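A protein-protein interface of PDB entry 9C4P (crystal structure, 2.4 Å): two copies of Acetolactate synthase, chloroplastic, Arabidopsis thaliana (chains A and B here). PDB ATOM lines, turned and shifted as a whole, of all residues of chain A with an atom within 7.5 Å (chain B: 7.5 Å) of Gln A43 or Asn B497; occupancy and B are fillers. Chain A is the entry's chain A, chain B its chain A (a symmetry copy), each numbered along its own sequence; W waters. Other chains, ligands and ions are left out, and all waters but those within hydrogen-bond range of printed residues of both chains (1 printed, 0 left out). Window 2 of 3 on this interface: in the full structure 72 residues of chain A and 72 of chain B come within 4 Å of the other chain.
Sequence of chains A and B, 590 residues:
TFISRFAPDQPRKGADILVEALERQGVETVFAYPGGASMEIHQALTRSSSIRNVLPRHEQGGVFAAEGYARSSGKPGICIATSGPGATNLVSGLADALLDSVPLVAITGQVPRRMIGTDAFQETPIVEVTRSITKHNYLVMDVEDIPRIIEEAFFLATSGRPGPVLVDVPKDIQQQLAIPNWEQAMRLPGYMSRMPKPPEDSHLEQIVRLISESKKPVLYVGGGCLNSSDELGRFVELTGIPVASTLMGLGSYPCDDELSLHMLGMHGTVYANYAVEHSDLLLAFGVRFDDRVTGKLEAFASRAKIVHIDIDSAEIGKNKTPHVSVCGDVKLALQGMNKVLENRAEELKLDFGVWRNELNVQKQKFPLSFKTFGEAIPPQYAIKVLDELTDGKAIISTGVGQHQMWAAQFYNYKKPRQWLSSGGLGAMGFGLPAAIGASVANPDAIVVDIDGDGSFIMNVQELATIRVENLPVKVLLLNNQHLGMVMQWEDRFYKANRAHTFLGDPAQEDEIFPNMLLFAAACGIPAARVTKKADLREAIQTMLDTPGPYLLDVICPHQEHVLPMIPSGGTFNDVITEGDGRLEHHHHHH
The side-chain amino group of Lys A13 lies within salt-bridge range of the side-chain carboxylate of Glu A40 (2.9 Å).
O of Gln A43 sits at hydrogen-bond distance from OG1 of Thr A46 (2.7 Å).
N of Ala B496 sits at hydrogen-bond distance from O of Glu B490, at 2.9 Å.
N of Ala B499 is in hydrogen-bond range of OE2 of Glu B490, at 2.7 Å.
The side-chain carboxylate (OE1) of Glu B490 is in hydrogen-bond range of the side-chain hydroxyl (OG1) of Thr B501 (2.9 Å).
The guanidinium group (NH1) of Arg B498 is in salt-bridge range of the side-chain carboxylate (OD1) of Asp B491, at 2.9 Å.
Hydrophobic or aromatic side chains of chain A within 4 Å of the printed part of chain B: Met A39 and His A42.
Hydrophobic or aromatic side chains of chain B within 4 Å of the printed part of chain A: Val B486, Trp B489, Tyr B494, Ala B499 and His B500.
Among the printed residues, no Asp or Glu carboxylate lies within 4 Å of a Lys or Arg side-chain nitrogen of the other chain.
Water W1 bridges the side-chain hydroxyl (OG1) of Thr A46 (2.9 Å) and the side-chain amide nitrogen (ND2) of Asn B497 (3.4 Å).
Printed residues of chain B within 4 Å of Gln A43: Glu B490 (3.98 Å), Tyr B494 (3.6 Å), Asn B497 (2.8 Å) and Ala B499 (3.7 Å).
Of chain A, only Gln A43 and Thr A46 come within 4 Å of Asn B497.
Of the printed residues of chain B, His A42 touches Ala B499 (3.5 Å) and His B500 (3.0 Å).
Of the printed residues of chain A, Tyr B494 touches Met A39, Glu A40 and Gln A43.
Printed residues of chain A within 4 Å of Val B486: Met A39 (3.7 Å).
Printed residues of chain A within 4 Å of Ala B499: His A42 (3.5 Å), Gln A43 (3.7 Å) and Thr A46 (3.8 Å).
Of the printed residues of chain A, His B500 touches His A42.
The nearest residue of chain A that does not touch Asn B497 is Arg A47 (5.7 Å).
The side-chain hydroxyl (OH) of Tyr B494 sits at hydrogen-bond distance from the side-chain carboxylate (OE2) of Glu A40 (2.6 Å).
A ring nitrogen (ND1) of His A42 lies within hydrogen-bond range of a ring nitrogen (ND1) of His B500 (3.0 Å).
The side-chain amide oxygen (OE1) of Gln A43 lies within hydrogen-bond range of the side-chain amide nitrogen (ND2) of Asn B497 (2.8 Å).
OG1 of Thr A46 sits at hydrogen-bond distance from ND2 of Asn B497 (3.3 Å).
No position is printed for both chains.
Of the 14 pairs that touch across the chains among the printed residues, none has its exchanged pair printed and touching as well.
Among the printed residues, merely in contact across the chains: Met A39 with Val B486, Met A39 with Trp B489, Met A39 with Glu B490, Met A39 with Tyr B494, His A42 with Ala B499, Gln A43 with Glu B490, Gln A43 with Tyr B494, Gln A43 with Ala B499, Thr A46 with Arg B498 and Thr A46 with Ala B499.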
ATOM      1  N   ARG A   5       4.367 -34.005  -8.658  1.00  0.00           N
ATOM      2  CA  ARG A   5       4.155 -34.458  -7.291  1.00  0.00           C
ATOM      3  C   ARG A   5       3.053 -33.677  -6.588  1.00  0.00           C
ATOM      4  O   ARG A   5       2.791 -33.922  -5.406  1.00  0.00           O
ATOM      5  CB  ARG A   5       5.458 -34.358  -6.487  1.00  0.00           C
ATOM      6  CG  ARG A   5       6.674 -34.941  -7.202  1.00  0.00           C
ATOM      7  CD  ARG A   5       7.913 -34.935  -6.313  1.00  0.00           C
ATOM      8  NE  ARG A   5       8.082 -33.672  -5.602  1.00  0.00           N
ATOM      9  CZ  ARG A   5       8.786 -32.643  -6.052  1.00  0.00           C
ATOM     10  NH1 ARG A   5       9.400 -32.684  -7.224  1.00  0.00           N
ATOM     11  NH2 ARG A   5       8.879 -31.544  -5.307  1.00  0.00           N
ATOM     12  N   LYS A  13       4.654 -23.937  -2.725  1.00  0.00           N
ATOM     13  CA  LYS A  13       5.634 -22.866  -2.633  1.00  0.00           C
ATOM     14  C   LYS A  13       6.287 -22.618  -3.988  1.00  0.00           C
ATOM     15  O   LYS A  13       6.391 -23.515  -4.828  1.00  0.00           O
ATOM     16  CB  LYS A  13       6.706 -23.212  -1.601  1.00  0.00           C
ATOM     17  CG  LYS A  13       6.214 -23.289  -0.169  1.00  0.00           C
ATOM     18  CD  LYS A  13       7.358 -23.685   0.750  1.00  0.00           C
ATOM     19  CE  LYS A  13       6.966 -23.593   2.208  1.00  0.00           C
ATOM     20  NZ  LYS A  13       8.132 -23.849   3.100  1.00  0.00           N
ATOM     21  N   ALA A  15       9.353 -22.255  -4.457  1.00  0.00           N
ATOM     22  CA  ALA A  15      10.527 -23.119  -4.530  1.00  0.00           C
ATOM     23  C   ALA A  15      10.176 -24.477  -5.126  1.00  0.00           C
ATOM     24  O   ALA A  15      10.948 -25.036  -5.913  1.00  0.00           O
ATOM     25  CB  ALA A  15      11.147 -23.281  -3.142  1.00  0.00           C
ATOM     26  N   ASP A  16       9.009 -25.022  -4.765  1.00  0.00           N
ATOM     27  CA  ASP A  16       8.552 -26.270  -5.368  1.00  0.00           C
ATOM     28  C   ASP A  16       8.187 -26.083  -6.832  1.00  0.00           C
ATOM     29  O   ASP A  16       8.386 -26.995  -7.642  1.00  0.00           O
ATOM     30  CB  ASP A  16       7.358 -26.824  -4.590  1.00  0.00           C
ATOM     31  CG  ASP A  16       7.750 -27.362  -3.231  1.00  0.00           C
ATOM     32  OD1 ASP A  16       8.541 -28.326  -3.174  1.00  0.00           O
ATOM     33  OD2 ASP A  16       7.274 -26.813  -2.217  1.00  0.00           O
ATOM     34  N   VAL A  19      11.607 -26.116  -8.616  1.00  0.00           N
ATOM     35  CA  VAL A  19      12.198 -27.448  -8.729  1.00  0.00           C
ATOM     36  C   VAL A  19      11.459 -28.274  -9.776  1.00  0.00           C
ATOM     37  O   VAL A  19      12.082 -28.959 -10.596  1.00  0.00           O
ATOM     38  CB  VAL A  19      12.219 -28.148  -7.357  1.00  0.00           C
ATOM     39  CG1 VAL A  19      12.579 -29.621  -7.513  1.00  0.00           C
ATOM     40  CG2 VAL A  19      13.212 -27.461  -6.438  1.00  0.00           C
ATOM     41  N   SER A  38      18.378 -19.227  -0.039  1.00  0.00           N
ATOM     42  CA  SER A  38      17.983 -20.341  -0.895  1.00  0.00           C
ATOM     43  C   SER A  38      17.566 -21.577  -0.104  1.00  0.00           C
ATOM     44  O   SER A  38      17.441 -22.658  -0.695  1.00  0.00           O
ATOM     45  CB  SER A  38      19.114 -20.699  -1.866  1.00  0.00           C
ATOM     46  OG  SER A  38      20.258 -21.187  -1.180  1.00  0.00           O
ATOM     47  N   MET A  39      17.345 -21.449   1.209  1.00  0.00           N
ATOM     48  CA  MET A  39      16.933 -22.595   2.018  1.00  0.00           C
ATOM     49  C   MET A  39      15.667 -23.241   1.472  1.00  0.00           C
ATOM     50  O   MET A  39      15.552 -24.472   1.446  1.00  0.00           O
ATOM     51  CB  MET A  39      16.713 -22.172   3.471  1.00  0.00           C
ATOM     52  CG  MET A  39      17.981 -21.905   4.255  1.00  0.00           C
ATOM     53  SD  MET A  39      17.666 -21.801   6.023  1.00  0.00           S
ATOM     54  CE  MET A  39      17.231 -23.504   6.384  1.00  0.00           C
ATOM     55  N   GLU A  40      14.702 -22.424   1.037  1.00  0.00           N
ATOM     56  CA  GLU A  40      13.453 -22.963   0.507  1.00  0.00           C
ATOM     57  C   GLU A  40      13.701 -23.822  -0.726  1.00  0.00           C
ATOM     58  O   GLU A  40      13.087 -24.883  -0.889  1.00  0.00           O
ATOM     59  CB  GLU A  40      12.489 -21.822   0.179  1.00  0.00           C
ATOM     60  CG  GLU A  40      12.039 -21.015   1.386  1.00  0.00           C
ATOM     61  CD  GLU A  40      10.994 -21.739   2.212  1.00  0.00           C
ATOM     62  OE1 GLU A  40      10.380 -22.694   1.689  1.00  0.00           O
ATOM     63  OE2 GLU A  40      10.789 -21.352   3.384  1.00  0.00           O
ATOM     64  N   ILE A  41      14.594 -23.376  -1.609  1.00  0.00           N
ATOM     65  CA  ILE A  41      14.921 -24.161  -2.796  1.00  0.00           C
ATOM     66  C   ILE A  41      15.546 -25.491  -2.395  1.00  0.00           C
ATOM     67  O   ILE A  41      15.263 -26.535  -2.996  1.00  0.00           O
ATOM     68  CB  ILE A  41      15.843 -23.352  -3.728  1.00  0.00           C
ATOM     69  CG1 ILE A  41      15.096 -22.130  -4.273  1.00  0.00           C
ATOM     70  CG2 ILE A  41      16.375 -24.225  -4.858  1.00  0.00           C
ATOM     71  CD1 ILE A  41      15.987 -21.133  -4.987  1.00  0.00           C
ATOM     72  N   HIS A  42      16.390 -25.478  -1.360  1.00  0.00           N
ATOM     73  CA  HIS A  42      17.043 -26.710  -0.932  1.00  0.00           C
ATOM     74  C   HIS A  42      16.054 -27.661  -0.270  1.00  0.00           C
ATOM     75  O   HIS A  42      16.143 -28.881  -0.455  1.00  0.00           O
ATOM     76  CB  HIS A  42      18.211 -26.386  -0.002  1.00  0.00           C
ATOM     77  CG  HIS A  42      19.455 -25.985  -0.730  1.00  0.00           C
ATOM     78  ND1 HIS A  42      20.508 -26.850  -0.935  1.00  0.00           N
ATOM     79  CD2 HIS A  42      19.801 -24.822  -1.331  1.00  0.00           C
ATOM     80  CE1 HIS A  42      21.457 -26.232  -1.615  1.00  0.00           C
ATOM     81  NE2 HIS A  42      21.052 -25.001  -1.870  1.00  0.00           N
ATOM     82  N   GLN A  43      15.103 -27.125   0.501  1.00  0.00           N
ATOM     83  CA  GLN A  43      14.035 -27.964   1.036  1.00  0.00           C
ATOM     84  C   GLN A  43      13.228 -28.604  -0.087  1.00  0.00           C
ATOM     85  O   GLN A  43      12.898 -29.794  -0.024  1.00  0.00           O
ATOM     86  CB  GLN A  43      13.124 -27.143   1.950  1.00  0.00           C
ATOM     87  CG  GLN A  43      13.770 -26.728   3.261  1.00  0.00           C
ATOM     88  CD  GLN A  43      14.039 -27.909   4.174  1.00  0.00           C
ATOM     89  OE1 GLN A  43      13.232 -28.833   4.265  1.00  0.00           O
ATOM     90  NE2 GLN A  43      15.182 -27.886   4.850  1.00  0.00           N
ATOM     91  N   ALA A  44      12.910 -27.830  -1.130  1.00  0.00           N
ATOM     92  CA  ALA A  44      12.144 -28.374  -2.247  1.00  0.00           C
ATOM     93  C   ALA A  44      12.941 -29.409  -3.029  1.00  0.00           C
ATOM     94  O   ALA A  44      12.352 -30.309  -3.640  1.00  0.00           O
ATOM     95  CB  ALA A  44      11.689 -27.244  -3.171  1.00  0.00           C
ATOM     96  N   LEU A  45      14.273 -29.300  -3.024  1.00  0.00           N
ATOM     97  CA  LEU A  45      15.101 -30.282  -3.718  1.00  0.00           C
ATOM     98  C   LEU A  45      15.035 -31.647  -3.043  1.00  0.00           C
ATOM     99  O   LEU A  45      15.013 -32.680  -3.724  1.00  0.00           O
ATOM    100  CB  LEU A  45      16.547 -29.794  -3.789  1.00  0.00           C
ATOM    101  CG  LEU A  45      16.887 -28.729  -4.830  1.00  0.00           C
ATOM    102  CD1 LEU A  45      18.332 -28.292  -4.666  1.00  0.00           C
ATOM    103  CD2 LEU A  45      16.640 -29.261  -6.237  1.00  0.00           C
ATOM    104  N   THR A  46      15.017 -31.677  -1.706  1.00  0.00           N
ATOM    105  CA  THR A  46      14.895 -32.950  -1.004  1.00  0.00           C
ATOM    106  C   THR A  46      13.556 -33.620  -1.273  1.00  0.00           C
ATOM    107  O   THR A  46      13.455 -34.846  -1.161  1.00  0.00           O
ATOM    108  CB  THR A  46      15.080 -32.761   0.505  1.00  0.00           C
ATOM    109  OG1 THR A  46      13.999 -31.981   1.032  1.00  0.00           O
ATOM    110  CG2 THR A  46      16.397 -32.062   0.800  1.00  0.00           C
ATOM    111  N   ARG A  47      12.529 -32.845  -1.627  1.00  0.00           N
ATOM    112  CA  ARG A  47      11.230 -33.406  -1.971  1.00  0.00           C
ATOM    113  C   ARG A  47      11.183 -33.956  -3.387  1.00  0.00           C
ATOM    114  O   ARG A  47      10.242 -34.684  -3.719  1.00  0.00           O
ATOM    115  CB  ARG A  47      10.133 -32.353  -1.786  1.00  0.00           C
ATOM    116  CG  ARG A  47       9.915 -31.953  -0.334  1.00  0.00           C
ATOM    117  CD  ARG A  47       8.673 -31.091  -0.163  1.00  0.00           C
ATOM    118  NE  ARG A  47       8.876 -29.714  -0.597  1.00  0.00           N
ATOM    119  CZ  ARG A  47       9.296 -28.734   0.193  1.00  0.00           C
ATOM    120  NH1 ARG A  47       9.596 -28.951   1.464  1.00  0.00           N
ATOM    121  NH2 ARG A  47       9.415 -27.504  -0.303  1.00  0.00           N
ATOM    122  N   SER A  48      12.163 -33.632  -4.225  1.00  0.00           N
ATOM    123  CA  SER A  48      12.231 -34.190  -5.569  1.00  0.00           C
ATOM    124  C   SER A  48      12.923 -35.544  -5.530  1.00  0.00           C
ATOM    125  O   SER A  48      13.975 -35.696  -4.900  1.00  0.00           O
ATOM    126  CB  SER A  48      12.981 -33.246  -6.506  1.00  0.00           C
ATOM    127  OG  SER A  48      13.233 -33.873  -7.755  1.00  0.00           O
ATOM    128  N   VAL B 486      22.872 -22.693   9.010  1.00  0.00           N
ATOM    129  CA  VAL B 486      21.771 -23.165   8.177  1.00  0.00           C
ATOM    130  C   VAL B 486      21.097 -24.366   8.830  1.00  0.00           C
ATOM    131  O   VAL B 486      19.872 -24.526   8.760  1.00  0.00           O
ATOM    132  CB  VAL B 486      22.272 -23.495   6.758  1.00  0.00           C
ATOM    133  CG1 VAL B 486      21.123 -23.985   5.888  1.00  0.00           C
ATOM    134  CG2 VAL B 486      22.929 -22.275   6.136  1.00  0.00           C
ATOM    135  N   MET B 487      21.888 -25.222   9.484  1.00  0.00           N
ATOM    136  CA  MET B 487      21.330 -26.339  10.241  1.00  0.00           C
ATOM    137  C   MET B 487      20.406 -25.849  11.352  1.00  0.00           C
ATOM    138  O   MET B 487      19.335 -26.426  11.580  1.00  0.00           O
ATOM    139  CB  MET B 487      22.465 -27.186  10.819  1.00  0.00           C
ATOM    140  CG  MET B 487      22.015 -28.331  11.714  1.00  0.00           C
ATOM    141  SD  MET B 487      23.120 -28.562  13.125  1.00  0.00           S
ATOM    142  CE  MET B 487      22.828 -27.039  14.027  1.00  0.00           C
ATOM    143  N   TRP B 489      18.603 -23.126  11.425  1.00  0.00           N
ATOM    144  CA  TRP B 489      17.336 -22.697  10.843  1.00  0.00           C
ATOM    145  C   TRP B 489      16.511 -23.885  10.366  1.00  0.00           C
ATOM    146  O   TRP B 489      15.276 -23.842  10.426  1.00  0.00           O
ATOM    147  CB  TRP B 489      17.592 -21.709   9.705  1.00  0.00           C
ATOM    148  CG  TRP B 489      17.822 -20.314  10.202  1.00  0.00           C
ATOM    149  CD1 TRP B 489      18.802 -19.903  11.060  1.00  0.00           C
ATOM    150  CD2 TRP B 489      17.054 -19.147   9.881  1.00  0.00           C
ATOM    151  NE1 TRP B 489      18.689 -18.554  11.296  1.00  0.00           N
ATOM    152  CE2 TRP B 489      17.625 -18.066  10.583  1.00  0.00           C
ATOM    153  CE3 TRP B 489      15.939 -18.911   9.070  1.00  0.00           C
ATOM    154  CZ2 TRP B 489      17.119 -16.769  10.498  1.00  0.00           C
ATOM    155  CZ3 TRP B 489      15.439 -17.621   8.985  1.00  0.00           C
ATOM    156  CH2 TRP B 489      16.029 -16.568   9.694  1.00  0.00           C
ATOM    157  N   GLU B 490      17.167 -24.949   9.893  1.00  0.00           N
ATOM    158  CA  GLU B 490      16.446 -26.180   9.587  1.00  0.00           C
ATOM    159  C   GLU B 490      15.736 -26.719  10.824  1.00  0.00           C
ATOM    160  O   GLU B 490      14.571 -27.127  10.750  1.00  0.00           O
ATOM    161  CB  GLU B 490      17.408 -27.224   9.016  1.00  0.00           C
ATOM    162  CG  GLU B 490      17.909 -26.896   7.614  1.00  0.00           C
ATOM    163  CD  GLU B 490      18.934 -27.894   7.091  1.00  0.00           C
ATOM    164  OE1 GLU B 490      19.644 -28.521   7.908  1.00  0.00           O
ATOM    165  OE2 GLU B 490      19.030 -28.048   5.855  1.00  0.00           O
ATOM    166  N   ASP B 491      16.415 -26.707  11.976  1.00  0.00           N
ATOM    167  CA  ASP B 491      15.807 -27.208  13.207  1.00  0.00           C
ATOM    168  C   ASP B 491      14.624 -26.349  13.638  1.00  0.00           C
ATOM    169  O   ASP B 491      13.581 -26.878  14.038  1.00  0.00           O
ATOM    170  CB  ASP B 491      16.849 -27.264  14.326  1.00  0.00           C
ATOM    171  CG  ASP B 491      17.962 -28.253  14.042  1.00  0.00           C
ATOM    172  OD1 ASP B 491      17.780 -29.121  13.162  1.00  0.00           O
ATOM    173  OD2 ASP B 491      19.015 -28.168  14.709  1.00  0.00           O
ATOM    174  N   PHE B 493      12.741 -24.005  11.848  1.00  0.00           N
ATOM    175  CA  PHE B 493      11.679 -23.635  10.927  1.00  0.00           C
ATOM    176  C   PHE B 493      11.352 -24.685   9.877  1.00  0.00           C
ATOM    177  O   PHE B 493      10.378 -24.503   9.139  1.00  0.00           O
ATOM    178  CB  PHE B 493      12.036 -22.311  10.228  1.00  0.00           C
ATOM    179  CG  PHE B 493      12.489 -21.235  11.180  1.00  0.00           C
ATOM    180  CD1 PHE B 493      11.594 -20.657  12.068  1.00  0.00           C
ATOM    181  CD2 PHE B 493      13.809 -20.807  11.195  1.00  0.00           C
ATOM    182  CE1 PHE B 493      12.005 -19.671  12.952  1.00  0.00           C
ATOM    183  CE2 PHE B 493      14.226 -19.820  12.076  1.00  0.00           C
ATOM    184  CZ  PHE B 493      13.322 -19.252  12.957  1.00  0.00           C
ATOM    185  N   TYR B 494      12.112 -25.778   9.790  1.00  0.00           N
ATOM    186  CA  TYR B 494      11.860 -26.800   8.780  1.00  0.00           C
ATOM    187  C   TYR B 494      11.854 -28.199   9.388  1.00  0.00           C
ATOM    188  O   TYR B 494      12.158 -29.180   8.702  1.00  0.00           O
ATOM    189  CB  TYR B 494      12.878 -26.706   7.644  1.00  0.00           C
ATOM    190  CG  TYR B 494      12.852 -25.370   6.936  1.00  0.00           C
ATOM    191  CD1 TYR B 494      11.974 -25.137   5.883  1.00  0.00           C
ATOM    192  CD2 TYR B 494      13.696 -24.337   7.326  1.00  0.00           C
ATOM    193  CE1 TYR B 494      11.943 -23.916   5.235  1.00  0.00           C
ATOM    194  CE2 TYR B 494      13.672 -23.112   6.685  1.00  0.00           C
ATOM    195  CZ  TYR B 494      12.794 -22.907   5.640  1.00  0.00           C
ATOM    196  OH  TYR B 494      12.766 -21.687   5.001  1.00  0.00           O
ATOM    197  N   LYS B 495      11.507 -28.302  10.675  1.00  0.00           N
ATOM    198  CA  LYS B 495      11.336 -29.587  11.360  1.00  0.00           C
ATOM    199  C   LYS B 495      12.595 -30.450  11.264  1.00  0.00           C
ATOM    200  O   LYS B 495      12.519 -31.670  11.108  1.00  0.00           O
ATOM    201  CB  LYS B 495      10.122 -30.345  10.817  1.00  0.00           C
ATOM    202  CG  LYS B 495       8.811 -29.575  10.876  1.00  0.00           C
ATOM    203  CD  LYS B 495       7.639 -30.473  10.504  1.00  0.00           C
ATOM    204  CE  LYS B 495       6.337 -29.694  10.377  1.00  0.00           C
ATOM    205  NZ  LYS B 495       6.311 -28.843   9.153  1.00  0.00           N
ATOM    206  N   ALA B 496      13.759 -29.805  11.349  1.00  0.00           N
ATOM    207  CA  ALA B 496      15.063 -30.467  11.314  1.00  0.00           C
ATOM    208  C   ALA B 496      15.280 -31.286  10.044  1.00  0.00           C
ATOM    209  O   ALA B 496      16.101 -32.209  10.030  1.00  0.00           O
ATOM    210  CB  ALA B 496      15.273 -31.349  12.551  1.00  0.00           C
ATOM    211  N   ASN B 497      14.564 -30.972   8.967  1.00  0.00           N
ATOM    212  CA  ASN B 497      14.791 -31.650   7.697  1.00  0.00           C
ATOM    213  C   ASN B 497      16.092 -31.147   7.079  1.00  0.00           C
ATOM    214  O   ASN B 497      16.213 -29.963   6.743  1.00  0.00           O
ATOM    215  CB  ASN B 497      13.615 -31.421   6.752  1.00  0.00           C
ATOM    216  CG  ASN B 497      13.726 -32.236   5.477  1.00  0.00           C
ATOM    217  OD1 ASN B 497      13.743 -33.466   5.518  1.00  0.00           O
ATOM    218  ND2 ASN B 497      13.790 -31.556   4.337  1.00  0.00           N
ATOM    219  N   ARG B 498      17.064 -32.044   6.936  1.00  0.00           N
ATOM    220  CA  ARG B 498      18.394 -31.679   6.460  1.00  0.00           C
ATOM    221  C   ARG B 498      18.387 -31.537   4.943  1.00  0.00           C
ATOM    222  O   ARG B 498      18.030 -32.478   4.224  1.00  0.00           O
ATOM    223  CB  ARG B 498      19.418 -32.725   6.895  1.00  0.00           C
ATOM    224  CG  ARG B 498      19.628 -32.804   8.400  1.00  0.00           C
ATOM    225  CD  ARG B 498      20.472 -31.645   8.907  1.00  0.00           C
ATOM    226  NE  ARG B 498      20.595 -31.666  10.360  1.00  0.00           N
ATOM    227  CZ  ARG B 498      19.861 -30.931  11.184  1.00  0.00           C
ATOM    228  NH1 ARG B 498      18.965 -30.069  10.731  1.00  0.00           N
ATOM    229  NH2 ARG B 498      20.037 -31.059  12.497  1.00  0.00           N
ATOM    230  N   ALA B 499      18.790 -30.365   4.457  1.00  0.00           N
ATOM    231  CA  ALA B 499      18.909 -30.094   3.026  1.00  0.00           C
ATOM    232  C   ALA B 499      20.352 -29.683   2.748  1.00  0.00           C
ATOM    233  O   ALA B 499      20.655 -28.502   2.561  1.00  0.00           O
ATOM    234  CB  ALA B 499      17.907 -29.018   2.576  1.00  0.00           C
ATOM    235  N   HIS B 500      21.246 -30.677   2.749  1.00  0.00           N
ATOM    236  CA  HIS B 500      22.632 -30.524   2.296  1.00  0.00           C
ATOM    237  C   HIS B 500      23.453 -29.647   3.240  1.00  0.00           C
ATOM    238  O   HIS B 500      24.251 -28.818   2.802  1.00  0.00           O
ATOM    239  CB  HIS B 500      22.682 -29.982   0.864  1.00  0.00           C
ATOM    240  CG  HIS B 500      21.617 -30.546  -0.023  1.00  0.00           C
ATOM    241  ND1 HIS B 500      20.542 -29.802  -0.460  1.00  0.00           N
ATOM    242  CD2 HIS B 500      21.444 -31.789  -0.531  1.00  0.00           C
ATOM    243  CE1 HIS B 500      19.761 -30.558  -1.213  1.00  0.00           C
ATOM    244  NE2 HIS B 500      20.287 -31.768  -1.271  1.00  0.00           N
ATOM    245  N   THR B 501      23.269 -29.839   4.547  1.00  0.00           N
ATOM    246  CA  THR B 501      24.042 -29.118   5.548  1.00  0.00           C
ATOM    247  C   THR B 501      25.091 -29.975   6.242  1.00  0.00           C
ATOM    248  O   THR B 501      25.925 -29.427   6.970  1.00  0.00           O
ATOM    249  CB  THR B 501      23.111 -28.502   6.605  1.00  0.00           C
ATOM    250  OG1 THR B 501      22.213 -29.503   7.101  1.00  0.00           O
ATOM    251  CG2 THR B 501      22.308 -27.360   6.002  1.00  0.00           C
HETATM  252  O   HOH W   1      12.059 -33.734   2.376  1.00  0.00           O
